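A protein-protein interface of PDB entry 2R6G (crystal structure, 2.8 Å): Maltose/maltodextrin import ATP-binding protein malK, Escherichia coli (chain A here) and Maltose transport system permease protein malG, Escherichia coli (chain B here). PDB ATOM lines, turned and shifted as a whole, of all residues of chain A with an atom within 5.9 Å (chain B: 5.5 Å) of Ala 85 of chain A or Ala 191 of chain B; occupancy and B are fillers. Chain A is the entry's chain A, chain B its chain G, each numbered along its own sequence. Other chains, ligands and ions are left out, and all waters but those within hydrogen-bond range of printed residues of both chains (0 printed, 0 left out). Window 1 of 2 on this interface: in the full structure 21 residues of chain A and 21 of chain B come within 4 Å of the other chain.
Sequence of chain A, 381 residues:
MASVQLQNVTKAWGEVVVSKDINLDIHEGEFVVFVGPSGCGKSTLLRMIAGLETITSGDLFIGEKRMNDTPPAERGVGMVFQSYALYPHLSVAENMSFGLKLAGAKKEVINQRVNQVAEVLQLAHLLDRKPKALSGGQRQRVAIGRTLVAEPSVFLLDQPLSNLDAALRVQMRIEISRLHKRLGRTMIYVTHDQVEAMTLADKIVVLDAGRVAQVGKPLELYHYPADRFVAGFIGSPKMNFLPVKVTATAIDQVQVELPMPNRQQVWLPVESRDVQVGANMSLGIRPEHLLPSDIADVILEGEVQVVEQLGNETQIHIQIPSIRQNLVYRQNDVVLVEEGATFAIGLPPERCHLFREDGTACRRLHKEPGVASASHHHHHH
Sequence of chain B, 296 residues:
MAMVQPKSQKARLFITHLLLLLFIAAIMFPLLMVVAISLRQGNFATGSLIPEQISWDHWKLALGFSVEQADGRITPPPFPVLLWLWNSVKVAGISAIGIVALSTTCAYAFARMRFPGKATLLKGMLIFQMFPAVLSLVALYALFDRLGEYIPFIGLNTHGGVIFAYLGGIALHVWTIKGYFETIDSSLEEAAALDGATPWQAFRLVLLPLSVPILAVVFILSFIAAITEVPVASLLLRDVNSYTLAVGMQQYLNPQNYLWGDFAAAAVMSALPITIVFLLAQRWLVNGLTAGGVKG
Among the printed residues, merely in contact across the chains: Leu 86 of chain A with Leu 188 of chain B (3.1 Å), Phe 98 of chain A with Asp 195 of chain B (3.4 Å), Tyr 87 of chain A with Leu 188 of chain B (3.4 Å), Leu 52 of chain A with Glu 190 of chain B (3.5 Å), Arg 146 of chain A with Ala 191 of chain B (3.5 Å), Tyr 84 of chain A with Lys 295 of chain B (3.5 Å), Ser 83 of chain A with Val 294 of chain B (3.6 Å), Tyr 84 of chain A with Gly 293 of chain B (3.7 Å), Ala 85 of chain A with Leu 188 of chain B (3.7 Å), Ala 85 of chain A with Ala 191 of chain B (3.7 Å), Arg 146 of chain A with Asp 195 of chain B (3.8 Å), Phe 81 of chain A with Leu 194 of chain B (3.8 Å), Leu 52 of chain A with Leu 194 of chain B (3.9 Å), Ala 85 of chain A with Ser 187 of chain B (3.9 Å) and Phe 81 of chain A with Ala 191 of chain B (3.97 Å).
Of the 10 printed residues of chain A, 9 touch a printed residue of chain B.
Among the printed residues, 21 pairs touch across the chains.
The backbone NH of Tyr 87 of chain A is in hydrogen-bond range of the side-chain amide oxygen of Asn 95 of chain A.
The backbone carbonyl oxygen (O) of Ala 85 of chain A sits at hydrogen-bond distance from the guanidinium group (NH2) of Arg 146 of chain A (2.6 Å).
NH2 of Arg 146 of chain A is in hydrogen-bond range of O of Tyr 84 of chain A (3.0 Å).
N of Lys 295 of chain B lies within hydrogen-bond range of OG of Ser 83 of chain A, 2.9 Å away.
The side-chain carboxylate (OD2) of Asp 195 of chain B lies within hydrogen-bond range of the side-chain hydroxyl (OH) of Tyr 87 of chain A (3.1 Å).
The backbone NH (N) of Leu 86 of chain A lies within hydrogen-bond range of the backbone carbonyl oxygen (O) of Gly 293 of chain B, at 3.0 Å.
OH of Tyr 87 of chain A is in hydrogen-bond range of N of Ala 192 of chain B (3.2 Å).
N of Ala 85 of chain A lies within hydrogen-bond range of O of Gly 293 of chain B, 3.0 Å away.
O of Ala 191 of chain B is in hydrogen-bond range of OH of Tyr 87 of chain A.
Of the printed residues of chain B, Leu 52 of chain A touches Glu 190 and Leu 194.
Of the printed residues of chain B, Ser 83 of chain A touches Val 294 and Lys 295.
Of the printed residues of chain B, Leu 86 of chain A touches Leu 188 (3.1 Å) and Gly 293 (3.0 Å).
Ala 191 of chain B touches just these residues of chain A: Phe 81 (3.97 Å), Ala 85 (3.7 Å), Tyr 87 (3.1 Å) and Arg 146 (3.5 Å).
Printed residues of chain A within 4 Å of Ala 192 of chain B: Tyr 87 (3.2 Å).
Gly 196 of chain B touches none of the printed residues of chain A.
Of the printed residues of chain A, Lys 295 of chain B touches Ser 83 (2.9 Å) and Tyr 84 (3.5 Å).
The nearest printed residue of chain A that does not touch Asp 195 of chain B is Asn 95 of chain A (4.6 Å).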
ATOM      1  N   LEU A  52      -2.836 -10.986  -3.696  1.00  0.00           N
ATOM      2  CA  LEU A  52      -4.177 -11.013  -4.271  1.00  0.00           C
ATOM      3  C   LEU A  52      -5.190 -11.459  -3.214  1.00  0.00           C
ATOM      4  O   LEU A  52      -6.399 -11.317  -3.399  1.00  0.00           O
ATOM      5  CB  LEU A  52      -4.222 -11.929  -5.498  1.00  0.00           C
ATOM      6  CG  LEU A  52      -3.127 -11.765  -6.565  1.00  0.00           C
ATOM      7  CD1 LEU A  52      -3.291 -12.802  -7.662  1.00  0.00           C
ATOM      8  CD2 LEU A  52      -3.094 -10.359  -7.160  1.00  0.00           C
ATOM      9  N   PHE A  81      -0.826 -18.556 -13.074  1.00  0.00           N
ATOM     10  CA  PHE A  81      -2.043 -18.966 -12.376  1.00  0.00           C
ATOM     11  C   PHE A  81      -2.455 -20.409 -12.668  1.00  0.00           C
ATOM     12  O   PHE A  81      -2.237 -20.914 -13.776  1.00  0.00           O
ATOM     13  CB  PHE A  81      -3.194 -18.028 -12.750  1.00  0.00           C
ATOM     14  CG  PHE A  81      -3.008 -16.609 -12.283  1.00  0.00           C
ATOM     15  CD1 PHE A  81      -2.169 -15.733 -12.969  1.00  0.00           C
ATOM     16  CD2 PHE A  81      -3.694 -16.138 -11.168  1.00  0.00           C
ATOM     17  CE1 PHE A  81      -2.004 -14.415 -12.543  1.00  0.00           C
ATOM     18  CE2 PHE A  81      -3.539 -14.827 -10.734  1.00  0.00           C
ATOM     19  CZ  PHE A  81      -2.691 -13.962 -11.421  1.00  0.00           C
ATOM     20  N   SER A  83      -5.510 -21.323 -12.852  1.00  0.00           N
ATOM     21  CA  SER A  83      -6.349 -20.966 -13.988  1.00  0.00           C
ATOM     22  C   SER A  83      -5.379 -20.751 -15.158  1.00  0.00           C
ATOM     23  O   SER A  83      -4.591 -21.644 -15.460  1.00  0.00           O
ATOM     24  CB  SER A  83      -7.146 -19.703 -13.665  1.00  0.00           C
ATOM     25  OG  SER A  83      -7.723 -19.151 -14.832  1.00  0.00           O
ATOM     26  N   TYR A  84      -5.435 -19.596 -15.817  1.00  0.00           N
ATOM     27  CA  TYR A  84      -4.331 -19.128 -16.668  1.00  0.00           C
ATOM     28  C   TYR A  84      -4.291 -17.599 -16.664  1.00  0.00           C
ATOM     29  O   TYR A  84      -3.232 -16.994 -16.857  1.00  0.00           O
ATOM     30  CB  TYR A  84      -4.407 -19.686 -18.104  1.00  0.00           C
ATOM     31  CG  TYR A  84      -4.372 -21.203 -18.180  1.00  0.00           C
ATOM     32  CD1 TYR A  84      -3.263 -21.924 -17.732  1.00  0.00           C
ATOM     33  CD2 TYR A  84      -5.459 -21.918 -18.682  1.00  0.00           C
ATOM     34  CE1 TYR A  84      -3.247 -23.315 -17.770  1.00  0.00           C
ATOM     35  CE2 TYR A  84      -5.444 -23.310 -18.737  1.00  0.00           C
ATOM     36  CZ  TYR A  84      -4.336 -24.001 -18.282  1.00  0.00           C
ATOM     37  OH  TYR A  84      -4.319 -25.377 -18.337  1.00  0.00           O
ATOM     38  N   ALA A  85      -5.459 -16.999 -16.419  1.00  0.00           N
ATOM     39  CA  ALA A  85      -5.652 -15.548 -16.354  1.00  0.00           C
ATOM     40  C   ALA A  85      -5.064 -14.804 -17.554  1.00  0.00           C
ATOM     41  O   ALA A  85      -4.591 -13.670 -17.424  1.00  0.00           O
ATOM     42  CB  ALA A  85      -5.110 -14.991 -15.040  1.00  0.00           C
ATOM     43  N   LEU A  86      -5.090 -15.452 -18.719  1.00  0.00           N
ATOM     44  CA  LEU A  86      -4.576 -14.855 -19.947  1.00  0.00           C
ATOM     45  C   LEU A  86      -5.495 -13.732 -20.403  1.00  0.00           C
ATOM     46  O   LEU A  86      -6.706 -13.820 -20.234  1.00  0.00           O
ATOM     47  CB  LEU A  86      -4.448 -15.906 -21.055  1.00  0.00           C
ATOM     48  CG  LEU A  86      -3.574 -17.151 -20.856  1.00  0.00           C
ATOM     49  CD1 LEU A  86      -3.474 -17.905 -22.167  1.00  0.00           C
ATOM     50  CD2 LEU A  86      -2.184 -16.805 -20.348  1.00  0.00           C
ATOM     51  N   TYR A  87      -4.917 -12.675 -20.967  1.00  0.00           N
ATOM     52  CA  TYR A  87      -5.712 -11.568 -21.485  1.00  0.00           C
ATOM     53  C   TYR A  87      -6.336 -11.994 -22.816  1.00  0.00           C
ATOM     54  O   TYR A  87      -5.634 -12.071 -23.832  1.00  0.00           O
ATOM     55  CB  TYR A  87      -4.861 -10.305 -21.650  1.00  0.00           C
ATOM     56  CG  TYR A  87      -3.961  -9.978 -20.467  1.00  0.00           C
ATOM     57  CD1 TYR A  87      -2.575  -9.940 -20.616  1.00  0.00           C
ATOM     58  CD2 TYR A  87      -4.494  -9.698 -19.207  1.00  0.00           C
ATOM     59  CE1 TYR A  87      -1.743  -9.639 -19.544  1.00  0.00           C
ATOM     60  CE2 TYR A  87      -3.666  -9.394 -18.126  1.00  0.00           C
ATOM     61  CZ  TYR A  87      -2.293  -9.366 -18.303  1.00  0.00           C
ATOM     62  OH  TYR A  87      -1.463  -9.067 -17.246  1.00  0.00           O
ATOM     63  N   ASN A  95       0.391 -10.963 -24.752  1.00  0.00           N
ATOM     64  CA  ASN A  95       0.312 -11.483 -23.392  1.00  0.00           C
ATOM     65  C   ASN A  95       1.693 -11.587 -22.762  1.00  0.00           C
ATOM     66  O   ASN A  95       1.892 -11.204 -21.609  1.00  0.00           O
ATOM     67  CB  ASN A  95      -0.370 -12.850 -23.379  1.00  0.00           C
ATOM     68  CG  ASN A  95      -1.857 -12.753 -23.143  1.00  0.00           C
ATOM     69  OD1 ASN A  95      -2.310 -12.710 -22.002  1.00  0.00           O
ATOM     70  ND2 ASN A  95      -2.629 -12.729 -24.221  1.00  0.00           N
ATOM     71  N   PHE A  98       3.206  -7.961 -22.475  1.00  0.00           N
ATOM     72  CA  PHE A  98       2.400  -6.999 -21.721  1.00  0.00           C
ATOM     73  C   PHE A  98       3.151  -6.416 -20.529  1.00  0.00           C
ATOM     74  O   PHE A  98       3.064  -5.218 -20.265  1.00  0.00           O
ATOM     75  CB  PHE A  98       1.095  -7.647 -21.247  1.00  0.00           C
ATOM     76  CG  PHE A  98       0.124  -6.682 -20.619  1.00  0.00           C
ATOM     77  CD1 PHE A  98      -0.677  -5.863 -21.413  1.00  0.00           C
ATOM     78  CD2 PHE A  98      -0.002  -6.603 -19.236  1.00  0.00           C
ATOM     79  CE1 PHE A  98      -1.581  -4.974 -20.839  1.00  0.00           C
ATOM     80  CE2 PHE A  98      -0.905  -5.718 -18.651  1.00  0.00           C
ATOM     81  CZ  PHE A  98      -1.694  -4.903 -19.455  1.00  0.00           C
ATOM     82  N   ARG A 146       4.511 -15.716 -20.018  1.00  0.00           N
ATOM     83  CA  ARG A 146       4.211 -14.381 -19.505  1.00  0.00           C
ATOM     84  C   ARG A 146       5.091 -14.018 -18.306  1.00  0.00           C
ATOM     85  O   ARG A 146       5.564 -12.884 -18.197  1.00  0.00           O
ATOM     86  CB  ARG A 146       2.735 -14.290 -19.113  1.00  0.00           C
ATOM     87  CG  ARG A 146       2.216 -12.870 -18.964  1.00  0.00           C
ATOM     88  CD  ARG A 146       1.168 -12.769 -17.872  1.00  0.00           C
ATOM     89  NE  ARG A 146      -0.092 -13.416 -18.230  1.00  0.00           N
ATOM     90  CZ  ARG A 146      -1.007 -13.816 -17.350  1.00  0.00           C
ATOM     91  NH1 ARG A 146      -0.816 -13.657 -16.043  1.00  0.00           N
ATOM     92  NH2 ARG A 146      -2.116 -14.391 -17.777  1.00  0.00           N
ATOM     93  N   SER B 187      -9.610 -12.267 -12.158  1.00  0.00           N
ATOM     94  CA  SER B 187      -8.229 -12.699 -12.386  1.00  0.00           C
ATOM     95  C   SER B 187      -7.455 -11.858 -13.403  1.00  0.00           C
ATOM     96  O   SER B 187      -6.255 -11.630 -13.231  1.00  0.00           O
ATOM     97  CB  SER B 187      -8.193 -14.173 -12.800  1.00  0.00           C
ATOM     98  OG  SER B 187      -8.724 -15.002 -11.781  1.00  0.00           O
ATOM     99  N   LEU B 188      -8.138 -11.406 -14.455  1.00  0.00           N
ATOM    100  CA  LEU B 188      -7.493 -10.650 -15.532  1.00  0.00           C
ATOM    101  C   LEU B 188      -6.863  -9.347 -15.043  1.00  0.00           C
ATOM    102  O   LEU B 188      -5.852  -8.896 -15.588  1.00  0.00           O
ATOM    103  CB  LEU B 188      -8.476 -10.354 -16.675  1.00  0.00           C
ATOM    104  CG  LEU B 188      -9.063 -11.467 -17.559  1.00  0.00           C
ATOM    105  CD1 LEU B 188      -8.100 -12.637 -17.734  1.00  0.00           C
ATOM    106  CD2 LEU B 188     -10.416 -11.952 -17.035  1.00  0.00           C
ATOM    107  N   GLU B 189      -7.467  -8.755 -14.016  1.00  0.00           N
ATOM    108  CA  GLU B 189      -6.972  -7.511 -13.436  1.00  0.00           C
ATOM    109  C   GLU B 189      -5.865  -7.774 -12.419  1.00  0.00           C
ATOM    110  O   GLU B 189      -4.957  -6.958 -12.256  1.00  0.00           O
ATOM    111  CB  GLU B 189      -8.122  -6.709 -12.817  1.00  0.00           C
ATOM    112  CG  GLU B 189      -9.117  -6.188 -13.852  1.00  0.00           C
ATOM    113  CD  GLU B 189     -10.300  -5.465 -13.238  1.00  0.00           C
ATOM    114  OE1 GLU B 189     -10.090  -4.464 -12.519  1.00  0.00           O
ATOM    115  OE2 GLU B 189     -11.445  -5.892 -13.492  1.00  0.00           O
ATOM    116  N   GLU B 190      -5.949  -8.922 -11.750  1.00  0.00           N
ATOM    117  CA  GLU B 190      -4.910  -9.375 -10.826  1.00  0.00           C
ATOM    118  C   GLU B 190      -3.626  -9.681 -11.586  1.00  0.00           C
ATOM    119  O   GLU B 190      -2.529  -9.379 -11.114  1.00  0.00           O
ATOM    120  CB  GLU B 190      -5.373 -10.619 -10.066  1.00  0.00           C
ATOM    121  CG  GLU B 190      -6.490 -10.356  -9.065  1.00  0.00           C
ATOM    122  CD  GLU B 190      -7.014 -11.619  -8.399  1.00  0.00           C
ATOM    123  OE1 GLU B 190      -6.569 -12.732  -8.760  1.00  0.00           O
ATOM    124  OE2 GLU B 190      -7.882 -11.495  -7.509  1.00  0.00           O
ATOM    125  N   ALA B 191      -3.782 -10.279 -12.766  1.00  0.00           N
ATOM    126  CA  ALA B 191      -2.668 -10.565 -13.661  1.00  0.00           C
ATOM    127  C   ALA B 191      -2.021  -9.272 -14.137  1.00  0.00           C
ATOM    128  O   ALA B 191      -0.796  -9.184 -14.242  1.00  0.00           O
ATOM    129  CB  ALA B 191      -3.144 -11.387 -14.845  1.00  0.00           C
ATOM    130  N   ALA B 192      -2.855  -8.273 -14.422  1.00  0.00           N
ATOM    131  CA  ALA B 192      -2.381  -6.946 -14.797  1.00  0.00           C
ATOM    132  C   ALA B 192      -1.607  -6.312 -13.646  1.00  0.00           C
ATOM    133  O   ALA B 192      -0.518  -5.772 -13.848  1.00  0.00           O
ATOM    134  CB  ALA B 192      -3.542  -6.064 -15.209  1.00  0.00           C
ATOM    135  N   ALA B 193      -2.173  -6.398 -12.444  1.00  0.00           N
ATOM    136  CA  ALA B 193      -1.543  -5.861 -11.241  1.00  0.00           C
ATOM    137  C   ALA B 193      -0.168  -6.485 -11.009  1.00  0.00           C
ATOM    138  O   ALA B 193       0.789  -5.783 -10.685  1.00  0.00           O
ATOM    139  CB  ALA B 193      -2.444  -6.073 -10.031  1.00  0.00           C
ATOM    140  N   LEU B 194      -0.074  -7.800 -11.197  1.00  0.00           N
ATOM    141  CA  LEU B 194       1.190  -8.516 -11.053  1.00  0.00           C
ATOM    142  C   LEU B 194       2.154  -8.244 -12.209  1.00  0.00           C
ATOM    143  O   LEU B 194       3.357  -8.481 -12.089  1.00  0.00           O
ATOM    144  CB  LEU B 194       0.949 -10.019 -10.884  1.00  0.00           C
ATOM    145  CG  LEU B 194       0.369 -10.457  -9.535  1.00  0.00           C
ATOM    146  CD1 LEU B 194      -0.053 -11.914  -9.582  1.00  0.00           C
ATOM    147  CD2 LEU B 194       1.357 -10.222  -8.395  1.00  0.00           C
ATOM    148  N   ASP B 195       1.623  -7.749 -13.325  1.00  0.00           N
ATOM    149  CA  ASP B 195       2.459  -7.268 -14.422  1.00  0.00           C
ATOM    150  C   ASP B 195       2.867  -5.810 -14.191  1.00  0.00           C
ATOM    151  O   ASP B 195       3.680  -5.263 -14.936  1.00  0.00           O
ATOM    152  CB  ASP B 195       1.753  -7.442 -15.775  1.00  0.00           C
ATOM    153  CG  ASP B 195       1.892  -8.856 -16.340  1.00  0.00           C
ATOM    154  OD1 ASP B 195       2.311  -9.775 -15.600  1.00  0.00           O
ATOM    155  OD2 ASP B 195       1.576  -9.050 -17.534  1.00  0.00           O
ATOM    156  N   GLY B 196       2.294  -5.193 -13.157  1.00  0.00           N
ATOM    157  CA  GLY B 196       2.698  -3.857 -12.716  1.00  0.00           C
ATOM    158  C   GLY B 196       1.818  -2.704 -13.164  1.00  0.00           C
ATOM    159  O   GLY B 196       2.246  -1.548 -13.139  1.00  0.00           O
ATOM    160  N   GLY B 293      -8.570 -17.245 -21.749  1.00  0.00           N
ATOM    161  CA  GLY B 293      -8.263 -16.396 -20.600  1.00  0.00           C
ATOM    162  C   GLY B 293      -8.364 -17.062 -19.240  1.00  0.00           C
ATOM    163  O   GLY B 293      -7.353 -17.482 -18.678  1.00  0.00           O
ATOM    164  N   VAL B 294      -9.578 -17.150 -18.700  1.00  0.00           N
ATOM    165  CA  VAL B 294      -9.782 -17.755 -17.380  1.00  0.00           C
ATOM    166  C   VAL B 294     -10.374 -19.165 -17.459  1.00  0.00           C
ATOM    167  O   VAL B 294     -11.410 -19.387 -18.090  1.00  0.00           O
ATOM    168  CB  VAL B 294     -10.627 -16.853 -16.438  1.00  0.00           C
ATOM    169  CG1 VAL B 294     -11.028 -17.604 -15.174  1.00  0.00           C
ATOM    170  CG2 VAL B 294      -9.852 -15.598 -16.069  1.00  0.00           C
ATOM    171  N   LYS B 295      -9.687 -20.103 -16.811  1.00  0.00           N
ATOM    172  CA  LYS B 295     -10.109 -21.493 -16.707  1.00  0.00           C
ATOM    173  C   LYS B 295     -11.017 -21.670 -15.488  1.00  0.00           C
ATOM    174  O   LYS B 295     -10.704 -21.186 -14.396  1.00  0.00           O
ATOM    175  CB  LYS B 295      -8.867 -22.381 -16.582  1.00  0.00           C
ATOM    176  CG  LYS B 295      -9.128 -23.872 -16.566  1.00  0.00           C
ATOM    177  CD  LYS B 295      -7.827 -24.630 -16.377  1.00  0.00           C
ATOM    178  CE  LYS B 295      -8.046 -26.124 -16.432  1.00  0.00           C
ATOM    179  NZ  LYS B 295      -6.767 -26.866 -16.303  1.00  0.00           N
